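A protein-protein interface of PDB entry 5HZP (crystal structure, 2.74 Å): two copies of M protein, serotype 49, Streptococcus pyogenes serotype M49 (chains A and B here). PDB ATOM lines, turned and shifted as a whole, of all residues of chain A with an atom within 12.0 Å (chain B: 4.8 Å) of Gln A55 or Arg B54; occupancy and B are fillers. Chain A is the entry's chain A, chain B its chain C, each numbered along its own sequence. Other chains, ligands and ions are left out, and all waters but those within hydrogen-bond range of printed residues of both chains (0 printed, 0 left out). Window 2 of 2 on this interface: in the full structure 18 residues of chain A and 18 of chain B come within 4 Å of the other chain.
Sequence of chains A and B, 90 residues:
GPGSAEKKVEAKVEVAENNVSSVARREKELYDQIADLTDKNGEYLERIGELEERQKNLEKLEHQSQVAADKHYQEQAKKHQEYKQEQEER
NH1 of Arg A54 is in hydrogen-bond range of OE1 of Gln B55.
The side-chain carboxylate (OE1) of Glu A52 lies within salt-bridge range of the guanidinium group (NH2) of Arg B47, at 3.9 Å.
The side-chain amide nitrogen of Gln A55 sits at hydrogen-bond distance from the backbone carbonyl oxygen of Leu B51, at 3.1 Å.
Among the printed residues, pairs that only touch across the chains: Ile A48 with Arg B47, Leu A51 with Leu B51, Leu A51 with Glu B52, Glu A52 with Leu B51, Gln A55 with Arg B54 and Gln A55 with Gln B55.
Printed residues of chain B within 4 Å of Ile A48: Arg B47.
Of the printed residues of chain B, Leu A51 touches Leu B51 (3.8 Å) and Glu B52 (3.7 Å).
Of the printed residues of chain B, Glu A52 touches Arg B47 (3.9 Å) and Leu B51 (3.8 Å).
Gln A55 touches just these residues of chain B: Leu B51 (3.1 Å), Arg B54 (3.0 Å) and Gln B55 (3.5 Å).
Glu A59 touches none of the printed residues of chain B.
Of the printed residues of chain A, Arg B47 touches Ile A48 and Glu A52.
No residue of chain A comes within 4 Å of Glu B50.
Of chain A, only Leu A51, Glu A52 and Gln A55 come within 4 Å of Leu B51.
Of the printed residues of chain A, Glu B52 touches Leu A51.
No residue of chain A comes within 4 Å of Glu B53.
Of chain A, only Gln A55 (3.0 Å) comes within 4 Å of Arg B54.
Of chain A, only Arg A54 (2.7 Å) and Gln A55 (3.5 Å) come within 4 Å of Gln B55.
No residue of chain A comes within 4 Å of Leu B58.
The nearest residue of chain B that does not touch Gln A55 is Leu B58 (4.4 Å).
The nearest printed residue of chain B that does not touch Arg A54 is Leu B58 (7.0 Å).
Printed residues of chain B that touch a printed residue of chain A: Arg B47, Leu B51, Glu B52, Arg B54 and Gln B55.
Hydrophobic or aromatic side chains of chain B that line the printed part of chain A: Leu B51.
Hydrophobic or aromatic side chains of chain A that line the printed part of chain B: Ile A48 and Leu A51.
Among the printed residues, 9 pairs touch across the chains.
Leu A51 touches its own counterpart, Leu B51.
Leu A51 touches Glu B52, and with the chains exchanged Glu A52 touches Leu B51.
Glu A52 touches Arg B47, but with the chains exchanged Arg A47 does not touch Glu B52 (4.8 Å).
Gln A55 touches Leu B51, but with the chains exchanged Leu A51 does not touch Gln B55 (4.1 Å).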
ATOM      1  N   GLU A  46      -8.221  -4.801  16.842  1.00  0.00           N
ATOM      2  CA  GLU A  46      -7.750  -3.643  17.569  1.00  0.00           C
ATOM      3  C   GLU A  46      -6.971  -2.805  16.574  1.00  0.00           C
ATOM      4  O   GLU A  46      -7.034  -1.579  16.588  1.00  0.00           O
ATOM      5  CB  GLU A  46      -6.871  -4.072  18.743  1.00  0.00           C
ATOM      6  CG  GLU A  46      -5.983  -3.018  19.336  1.00  0.00           C
ATOM      7  CD  GLU A  46      -6.712  -2.181  20.350  1.00  0.00           C
ATOM      8  OE1 GLU A  46      -7.702  -1.528  19.954  1.00  0.00           O
ATOM      9  OE2 GLU A  46      -6.304  -2.185  21.536  1.00  0.00           O
ATOM     10  N   ARG A  47      -6.251  -3.501  15.696  1.00  0.00           N
ATOM     11  CA  ARG A  47      -5.377  -2.869  14.726  1.00  0.00           C
ATOM     12  C   ARG A  47      -6.201  -2.392  13.548  1.00  0.00           C
ATOM     13  O   ARG A  47      -6.003  -1.282  13.061  1.00  0.00           O
ATOM     14  CB  ARG A  47      -4.266  -3.834  14.271  1.00  0.00           C
ATOM     15  CG  ARG A  47      -3.069  -3.172  13.526  1.00  0.00           C
ATOM     16  CD  ARG A  47      -1.713  -3.919  13.772  1.00  0.00           C
ATOM     17  NE  ARG A  47      -1.625  -5.266  13.178  1.00  0.00           N
ATOM     18  CZ  ARG A  47      -1.200  -6.369  13.813  1.00  0.00           C
ATOM     19  NH1 ARG A  47      -0.814  -6.320  15.089  1.00  0.00           N
ATOM     20  NH2 ARG A  47      -1.160  -7.535  13.165  1.00  0.00           N
ATOM     21  N   ILE A  48      -7.145  -3.208  13.094  1.00  0.00           N
ATOM     22  CA  ILE A  48      -7.941  -2.799  11.944  1.00  0.00           C
ATOM     23  C   ILE A  48      -8.949  -1.738  12.381  1.00  0.00           C
ATOM     24  O   ILE A  48      -9.557  -1.056  11.559  1.00  0.00           O
ATOM     25  CB  ILE A  48      -8.667  -3.994  11.240  1.00  0.00           C
ATOM     26  CG1 ILE A  48     -10.144  -4.078  11.619  1.00  0.00           C
ATOM     27  CG2 ILE A  48      -7.911  -5.336  11.423  1.00  0.00           C
ATOM     28  CD1 ILE A  48     -10.845  -5.262  10.927  1.00  0.00           C
ATOM     29  N   GLY A  49      -9.099  -1.564  13.683  1.00  0.00           N
ATOM     30  CA  GLY A  49      -9.933  -0.490  14.174  1.00  0.00           C
ATOM     31  C   GLY A  49      -9.198   0.826  14.025  1.00  0.00           C
ATOM     32  O   GLY A  49      -9.789   1.849  13.679  1.00  0.00           O
ATOM     33  N   GLU A  50      -7.895   0.789  14.276  1.00  0.00           N
ATOM     34  CA  GLU A  50      -7.098   1.996  14.308  1.00  0.00           C
ATOM     35  C   GLU A  50      -6.650   2.390  12.893  1.00  0.00           C
ATOM     36  O   GLU A  50      -6.451   3.577  12.608  1.00  0.00           O
ATOM     37  CB  GLU A  50      -5.892   1.820  15.227  1.00  0.00           C
ATOM     38  CG  GLU A  50      -4.769   1.024  14.593  1.00  0.00           C
ATOM     39  CD  GLU A  50      -3.547   0.900  15.484  1.00  0.00           C
ATOM     40  OE1 GLU A  50      -3.255   1.867  16.227  1.00  0.00           O
ATOM     41  OE2 GLU A  50      -2.881  -0.164  15.433  1.00  0.00           O
ATOM     42  N   LEU A  51      -6.500   1.411  12.003  1.00  0.00           N
ATOM     43  CA  LEU A  51      -6.172   1.728  10.616  1.00  0.00           C
ATOM     44  C   LEU A  51      -7.403   2.304   9.943  1.00  0.00           C
ATOM     45  O   LEU A  51      -7.321   3.325   9.270  1.00  0.00           O
ATOM     46  CB  LEU A  51      -5.662   0.505   9.857  1.00  0.00           C
ATOM     47  CG  LEU A  51      -4.319  -0.019  10.375  1.00  0.00           C
ATOM     48  CD1 LEU A  51      -3.717  -1.147   9.522  1.00  0.00           C
ATOM     49  CD2 LEU A  51      -3.361   1.132  10.511  1.00  0.00           C
ATOM     50  N   GLU A  52      -8.553   1.676  10.157  1.00  0.00           N
ATOM     51  CA  GLU A  52      -9.796   2.184   9.581  1.00  0.00           C
ATOM     52  C   GLU A  52     -10.084   3.591  10.072  1.00  0.00           C
ATOM     53  O   GLU A  52     -10.846   4.323   9.441  1.00  0.00           O
ATOM     54  CB  GLU A  52     -10.983   1.268   9.909  1.00  0.00           C
ATOM     55  CG  GLU A  52     -11.138   0.081   8.968  1.00  0.00           C
ATOM     56  CD  GLU A  52     -12.433  -0.690   9.182  1.00  0.00           C
ATOM     57  OE1 GLU A  52     -12.878  -1.356   8.217  1.00  0.00           O
ATOM     58  OE2 GLU A  52     -12.997  -0.644  10.306  1.00  0.00           O
ATOM     59  N   GLU A  53      -9.472   3.960  11.196  1.00  0.00           N
ATOM     60  CA  GLU A  53      -9.633   5.289  11.770  1.00  0.00           C
ATOM     61  C   GLU A  53      -8.761   6.345  11.056  1.00  0.00           C
ATOM     62  O   GLU A  53      -9.286   7.352  10.559  1.00  0.00           O
ATOM     63  CB  GLU A  53      -9.300   5.259  13.259  1.00  0.00           C
ATOM     64  CG  GLU A  53     -10.335   5.938  14.131  1.00  0.00           C
ATOM     65  CD  GLU A  53      -9.718   6.549  15.389  1.00  0.00           C
ATOM     66  OE1 GLU A  53      -9.492   5.805  16.372  1.00  0.00           O
ATOM     67  OE2 GLU A  53      -9.452   7.778  15.393  1.00  0.00           O
ATOM     68  N   ARG A  54      -7.441   6.129  11.043  1.00  0.00           N
ATOM     69  CA  ARG A  54      -6.531   6.960  10.261  1.00  0.00           C
ATOM     70  C   ARG A  54      -7.088   7.137   8.865  1.00  0.00           C
ATOM     71  O   ARG A  54      -7.321   8.236   8.408  1.00  0.00           O
ATOM     72  CB  ARG A  54      -5.148   6.341  10.152  1.00  0.00           C
ATOM     73  CG  ARG A  54      -4.223   6.614  11.277  1.00  0.00           C
ATOM     74  CD  ARG A  54      -2.903   5.937  10.963  1.00  0.00           C
ATOM     75  NE  ARG A  54      -2.224   5.442  12.159  1.00  0.00           N
ATOM     76  CZ  ARG A  54      -1.303   4.479  12.153  1.00  0.00           C
ATOM     77  NH1 ARG A  54      -0.954   3.898  11.011  1.00  0.00           N
ATOM     78  NH2 ARG A  54      -0.731   4.087  13.289  1.00  0.00           N
ATOM     79  N   GLN A  55      -7.338   6.032   8.192  1.00  0.00           N
ATOM     80  CA  GLN A  55      -7.791   6.094   6.820  1.00  0.00           C
ATOM     81  C   GLN A  55      -9.117   6.820   6.659  1.00  0.00           C
ATOM     82  O   GLN A  55      -9.549   7.088   5.546  1.00  0.00           O
ATOM     83  CB  GLN A  55      -7.886   4.689   6.251  1.00  0.00           C
ATOM     84  CG  GLN A  55      -6.561   3.958   6.312  1.00  0.00           C
ATOM     85  CD  GLN A  55      -6.413   3.035   5.144  1.00  0.00           C
ATOM     86  OE1 GLN A  55      -7.235   3.055   4.216  1.00  0.00           O
ATOM     87  NE2 GLN A  55      -5.368   2.215   5.167  1.00  0.00           N
ATOM     88  N   LYS A  56      -9.764   7.148   7.762  1.00  0.00           N
ATOM     89  CA  LYS A  56     -10.958   7.969   7.677  1.00  0.00           C
ATOM     90  C   LYS A  56     -10.549   9.421   7.863  1.00  0.00           C
ATOM     91  O   LYS A  56     -11.176  10.343   7.341  1.00  0.00           O
ATOM     92  CB  LYS A  56     -11.987   7.561   8.735  1.00  0.00           C
ATOM     93  CG  LYS A  56     -13.400   8.068   8.453  1.00  0.00           C
ATOM     94  CD  LYS A  56     -13.828   7.690   7.034  1.00  0.00           C
ATOM     95  CE  LYS A  56     -15.349   7.691   6.876  1.00  0.00           C
ATOM     96  NZ  LYS A  56     -15.794   6.956   5.645  1.00  0.00           N
ATOM     97  N   ASN A  57      -9.502   9.598   8.656  1.00  0.00           N
ATOM     98  CA  ASN A  57      -8.929  10.894   8.926  1.00  0.00           C
ATOM     99  C   ASN A  57      -8.197  11.389   7.677  1.00  0.00           C
ATOM    100  O   ASN A  57      -8.527  12.436   7.130  1.00  0.00           O
ATOM    101  CB  ASN A  57      -7.982  10.819  10.137  1.00  0.00           C
ATOM    102  CG  ASN A  57      -8.718  10.899  11.475  1.00  0.00           C
ATOM    103  OD1 ASN A  57      -9.929  11.111  11.519  1.00  0.00           O
ATOM    104  ND2 ASN A  57      -7.972  10.773  12.570  1.00  0.00           N
ATOM    105  N   LEU A  58      -7.223  10.614   7.224  1.00  0.00           N
ATOM    106  CA  LEU A  58      -6.543  10.879   5.977  1.00  0.00           C
ATOM    107  C   LEU A  58      -7.507  11.132   4.801  1.00  0.00           C
ATOM    108  O   LEU A  58      -7.225  11.954   3.945  1.00  0.00           O
ATOM    109  CB  LEU A  58      -5.608   9.723   5.628  1.00  0.00           C
ATOM    110  CG  LEU A  58      -4.410   9.408   6.519  1.00  0.00           C
ATOM    111  CD1 LEU A  58      -3.264   8.821   5.699  1.00  0.00           C
ATOM    112  CD2 LEU A  58      -3.948  10.628   7.264  1.00  0.00           C
ATOM    113  N   GLU A  59      -8.629  10.427   4.737  1.00  0.00           N
ATOM    114  CA  GLU A  59      -9.577  10.649   3.646  1.00  0.00           C
ATOM    115  C   GLU A  59     -10.133  12.070   3.736  1.00  0.00           C
ATOM    116  O   GLU A  59     -10.388  12.722   2.720  1.00  0.00           O
ATOM    117  CB  GLU A  59     -10.719   9.626   3.687  1.00  0.00           C
ATOM    118  CG  GLU A  59     -11.757   9.735   2.559  1.00  0.00           C
ATOM    119  CD  GLU A  59     -13.183   9.422   3.038  1.00  0.00           C
ATOM    120  OE1 GLU A  59     -13.490   9.702   4.220  1.00  0.00           O
ATOM    121  OE2 GLU A  59     -13.999   8.898   2.243  1.00  0.00           O
ATOM    122  N   LYS A  60     -10.296  12.558   4.959  1.00  0.00           N
ATOM    123  CA  LYS A  60     -10.912  13.858   5.166  1.00  0.00           C
ATOM    124  C   LYS A  60      -9.874  14.963   4.937  1.00  0.00           C
ATOM    125  O   LYS A  60     -10.162  15.975   4.314  1.00  0.00           O
ATOM    126  CB  LYS A  60     -11.524  13.958   6.571  1.00  0.00           C
ATOM    127  CG  LYS A  60     -12.476  15.154   6.750  1.00  0.00           C
ATOM    128  CD  LYS A  60     -13.321  15.070   8.029  1.00  0.00           C
ATOM    129  CE  LYS A  60     -14.470  14.025   7.921  1.00  0.00           C
ATOM    130  NZ  LYS A  60     -14.179  12.647   8.474  1.00  0.00           N
ATOM    131  N   LEU A  61      -8.668  14.746   5.440  1.00  0.00           N
ATOM    132  CA  LEU A  61      -7.559  15.650   5.207  1.00  0.00           C
ATOM    133  C   LEU A  61      -7.339  15.886   3.710  1.00  0.00           C
ATOM    134  O   LEU A  61      -7.400  17.022   3.250  1.00  0.00           O
ATOM    135  CB  LEU A  61      -6.291  15.097   5.852  1.00  0.00           C
ATOM    136  CG  LEU A  61      -5.794  15.902   7.044  1.00  0.00           C
ATOM    137  CD1 LEU A  61      -6.926  16.241   7.978  1.00  0.00           C
ATOM    138  CD2 LEU A  61      -4.671  15.191   7.763  1.00  0.00           C
ATOM    139  N   GLU A  62      -7.090  14.824   2.951  1.00  0.00           N
ATOM    140  CA  GLU A  62      -6.813  14.956   1.530  1.00  0.00           C
ATOM    141  C   GLU A  62      -7.973  15.648   0.860  1.00  0.00           C
ATOM    142  O   GLU A  62      -7.792  16.372  -0.112  1.00  0.00           O
ATOM    143  CB  GLU A  62      -6.554  13.593   0.876  1.00  0.00           C
ATOM    144  CG  GLU A  62      -6.139  13.645  -0.606  1.00  0.00           C
ATOM    145  CD  GLU A  62      -7.318  13.812  -1.571  1.00  0.00           C
ATOM    146  OE1 GLU A  62      -8.472  13.681  -1.115  1.00  0.00           O
ATOM    147  OE2 GLU A  62      -7.095  14.073  -2.780  1.00  0.00           O
ATOM    148  N   HIS A  63      -9.172  15.425   1.375  1.00  0.00           N
ATOM    149  CA  HIS A  63     -10.349  16.042   0.784  1.00  0.00           C
ATOM    150  C   HIS A  63     -10.308  17.532   0.969  1.00  0.00           C
ATOM    151  O   HIS A  63     -10.533  18.309   0.034  1.00  0.00           O
ATOM    152  CB  HIS A  63     -11.612  15.514   1.416  1.00  0.00           C
ATOM    153  CG  HIS A  63     -12.853  16.160   0.897  1.00  0.00           C
ATOM    154  ND1 HIS A  63     -13.553  17.108   1.610  1.00  0.00           N
ATOM    155  CD2 HIS A  63     -13.531  15.976  -0.259  1.00  0.00           C
ATOM    156  CE1 HIS A  63     -14.611  17.484   0.913  1.00  0.00           C
ATOM    157  NE2 HIS A  63     -14.620  16.810  -0.224  1.00  0.00           N
ATOM    158  N   GLN A  64     -10.035  17.916   2.206  1.00  0.00           N
ATOM    159  CA  GLN A  64      -9.940  19.304   2.580  1.00  0.00           C
ATOM    160  C   GLN A  64      -8.919  20.036   1.682  1.00  0.00           C
ATOM    161  O   GLN A  64      -9.242  21.057   1.097  1.00  0.00           O
ATOM    162  CB  GLN A  64      -9.583  19.410   4.061  1.00  0.00           C
ATOM    163  CG  GLN A  64     -10.794  19.376   4.982  1.00  0.00           C
ATOM    164  CD  GLN A  64     -10.422  19.548   6.455  1.00  0.00           C
ATOM    165  OE1 GLN A  64      -9.246  19.463   6.831  1.00  0.00           O
ATOM    166  NE2 GLN A  64     -11.431  19.797   7.297  1.00  0.00           N
ATOM    167  N   ARG B  47      -7.006  -8.496   6.422  1.00  0.00           N
ATOM    168  CA  ARG B  47      -7.542  -7.156   6.396  1.00  0.00           C
ATOM    169  C   ARG B  47      -6.435  -6.174   6.742  1.00  0.00           C
ATOM    170  O   ARG B  47      -6.283  -5.143   6.086  1.00  0.00           O
ATOM    171  CB  ARG B  47      -8.714  -7.030   7.364  1.00  0.00           C
ATOM    172  CG  ARG B  47      -9.339  -5.653   7.405  1.00  0.00           C
ATOM    173  CD  ARG B  47     -10.612  -5.593   6.594  1.00  0.00           C
ATOM    174  NE  ARG B  47     -10.959  -4.215   6.267  1.00  0.00           N
ATOM    175  CZ  ARG B  47     -10.701  -3.627   5.099  1.00  0.00           C
ATOM    176  NH1 ARG B  47     -10.097  -4.303   4.118  1.00  0.00           N
ATOM    177  NH2 ARG B  47     -11.065  -2.362   4.903  1.00  0.00           N
ATOM    178  N   GLU B  50      -4.427  -5.717   3.562  1.00  0.00           N
ATOM    179  CA  GLU B  50      -5.084  -4.778   2.660  1.00  0.00           C
ATOM    180  C   GLU B  50      -4.940  -3.360   3.173  1.00  0.00           C
ATOM    181  O   GLU B  50      -4.780  -2.434   2.392  1.00  0.00           O
ATOM    182  CB  GLU B  50      -6.589  -5.077   2.502  1.00  0.00           C
ATOM    183  CG  GLU B  50      -6.973  -6.487   2.138  1.00  0.00           C
ATOM    184  CD  GLU B  50      -6.782  -6.793   0.679  1.00  0.00           C
ATOM    185  OE1 GLU B  50      -6.623  -7.993   0.347  1.00  0.00           O
ATOM    186  OE2 GLU B  50      -6.800  -5.842  -0.133  1.00  0.00           O
ATOM    187  N   LEU B  51      -5.014  -3.189   4.486  1.00  0.00           N
ATOM    188  CA  LEU B  51      -5.048  -1.856   5.054  1.00  0.00           C
ATOM    189  C   LEU B  51      -3.647  -1.287   5.193  1.00  0.00           C
ATOM    190  O   LEU B  51      -3.396  -0.162   4.797  1.00  0.00           O
ATOM    191  CB  LEU B  51      -5.772  -1.861   6.401  1.00  0.00           C
ATOM    192  CG  LEU B  51      -7.163  -1.208   6.359  1.00  0.00           C
ATOM    193  CD1 LEU B  51      -7.896  -1.595   5.117  1.00  0.00           C
ATOM    194  CD2 LEU B  51      -8.003  -1.551   7.577  1.00  0.00           C
ATOM    195  N   GLU B  52      -2.726  -2.069   5.742  1.00  0.00           N
ATOM    196  CA  GLU B  52      -1.341  -1.613   5.856  1.00  0.00           C
ATOM    197  C   GLU B  52      -0.764  -1.283   4.482  1.00  0.00           C
ATOM    198  O   GLU B  52       0.152  -0.478   4.362  1.00  0.00           O
ATOM    199  CB  GLU B  52      -0.469  -2.664   6.553  1.00  0.00           C
ATOM    200  CG  GLU B  52      -0.700  -2.790   8.054  1.00  0.00           C
ATOM    201  CD  GLU B  52       0.530  -3.313   8.771  1.00  0.00           C
ATOM    202  OE1 GLU B  52       1.181  -4.254   8.251  1.00  0.00           O
ATOM    203  OE2 GLU B  52       0.856  -2.774   9.852  1.00  0.00           O
ATOM    204  N   GLU B  53      -1.320  -1.906   3.453  1.00  0.00           N
ATOM    205  CA  GLU B  53      -0.884  -1.713   2.088  1.00  0.00           C
ATOM    206  C   GLU B  53      -1.420  -0.371   1.580  1.00  0.00           C
ATOM    207  O   GLU B  53      -0.660   0.543   1.271  1.00  0.00           O
ATOM    208  CB  GLU B  53      -1.379  -2.866   1.223  1.00  0.00           C
ATOM    209  CG  GLU B  53      -0.736  -3.035  -0.133  1.00  0.00           C
ATOM    210  CD  GLU B  53      -1.724  -3.601  -1.164  1.00  0.00           C
ATOM    211  OE1 GLU B  53      -1.281  -4.268  -2.127  1.00  0.00           O
ATOM    212  OE2 GLU B  53      -2.953  -3.376  -1.011  1.00  0.00           O
ATOM    213  N   ARG B  54      -2.740  -0.287   1.491  1.00  0.00           N
ATOM    214  CA  ARG B  54      -3.478   0.928   1.186  1.00  0.00           C
ATOM    215  C   ARG B  54      -2.860   2.172   1.808  1.00  0.00           C
ATOM    216  O   ARG B  54      -2.651   3.177   1.143  1.00  0.00           O
ATOM    217  CB  ARG B  54      -4.898   0.768   1.689  1.00  0.00           C
ATOM    218  CG  ARG B  54      -5.902   1.642   1.071  1.00  0.00           C
ATOM    219  CD  ARG B  54      -7.234   1.377   1.694  1.00  0.00           C
ATOM    220  NE  ARG B  54      -7.822   0.149   1.181  1.00  0.00           N
ATOM    221  CZ  ARG B  54      -9.042  -0.260   1.492  1.00  0.00           C
ATOM    222  NH1 ARG B  54      -9.775   0.471   2.315  1.00  0.00           N
ATOM    223  NH2 ARG B  54      -9.532  -1.387   0.985  1.00  0.00           N
ATOM    224  N   GLN B  55      -2.543   2.096   3.088  1.00  0.00           N
ATOM    225  CA  GLN B  55      -2.009   3.251   3.798  1.00  0.00           C
ATOM    226  C   GLN B  55      -0.624   3.632   3.282  1.00  0.00           C
ATOM    227  O   GLN B  55      -0.136   4.723   3.538  1.00  0.00           O
ATOM    228  CB  GLN B  55      -1.956   2.962   5.298  1.00  0.00           C
ATOM    229  CG  GLN B  55      -1.786   4.175   6.169  1.00  0.00           C
ATOM    230  CD  GLN B  55      -1.436   3.788   7.583  1.00  0.00           C
ATOM    231  OE1 GLN B  55      -1.900   4.405   8.544  1.00  0.00           O
ATOM    232  NE2 GLN B  55      -0.609   2.751   7.725  1.00  0.00           N
ATOM    233  N   LYS B  56       0.011   2.716   2.566  1.00  0.00           N
ATOM    234  CA  LYS B  56       1.329   2.966   2.013  1.00  0.00           C
ATOM    235  C   LYS B  56       1.179   3.531   0.603  1.00  0.00           C
ATOM    236  O   LYS B  56       1.963   4.366   0.152  1.00  0.00           O
ATOM    237  CB  LYS B  56       2.156   1.675   2.017  1.00  0.00           C
ATOM    238  CG  LYS B  56       3.604   1.858   1.615  1.00  0.00           C
ATOM    239  CD  LYS B  56       4.457   0.663   2.021  1.00  0.00           C
ATOM    240  CE  LYS B  56       4.592   0.544   3.549  1.00  0.00           C
ATOM    241  NZ  LYS B  56       5.501  -0.575   3.985  1.00  0.00           N
ATOM    242  N   ASN B  57       0.153   3.059  -0.082  1.00  0.00           N
ATOM    243  CA  ASN B  57      -0.177   3.519  -1.405  1.00  0.00           C
ATOM    244  C   ASN B  57      -0.756   4.933  -1.367  1.00  0.00           C
ATOM    245  O   ASN B  57      -0.811   5.617  -2.383  1.00  0.00           O
ATOM    246  CB  ASN B  57      -1.177   2.572  -2.059  1.00  0.00           C
ATOM    247  CG  ASN B  57      -0.531   1.315  -2.590  1.00  0.00           C
ATOM    248  OD1 ASN B  57       0.680   1.130  -2.470  1.00  0.00           O
ATOM    249  ND2 ASN B  57      -1.337   0.437  -3.183  1.00  0.00           N
ATOM    250  N   LEU B  58      -1.222   5.353  -0.199  1.00  0.00           N
ATOM    251  CA  LEU B  58      -1.813   6.663  -0.066  1.00  0.00           C
ATOM    252  C   LEU B  58      -0.727   7.627   0.277  1.00  0.00           C
ATOM    253  O   LEU B  58      -0.689   8.735  -0.228  1.00  0.00           O
ATOM    254  CB  LEU B  58      -2.870   6.700   1.026  1.00  0.00           C
ATOM    255  CG  LEU B  58      -4.161   5.912   0.904  1.00  0.00           C
ATOM    256  CD1 LEU B  58      -4.942   6.196   2.166  1.00  0.00           C
ATOM    257  CD2 LEU B  58      -4.935   6.296  -0.346  1.00  0.00           C
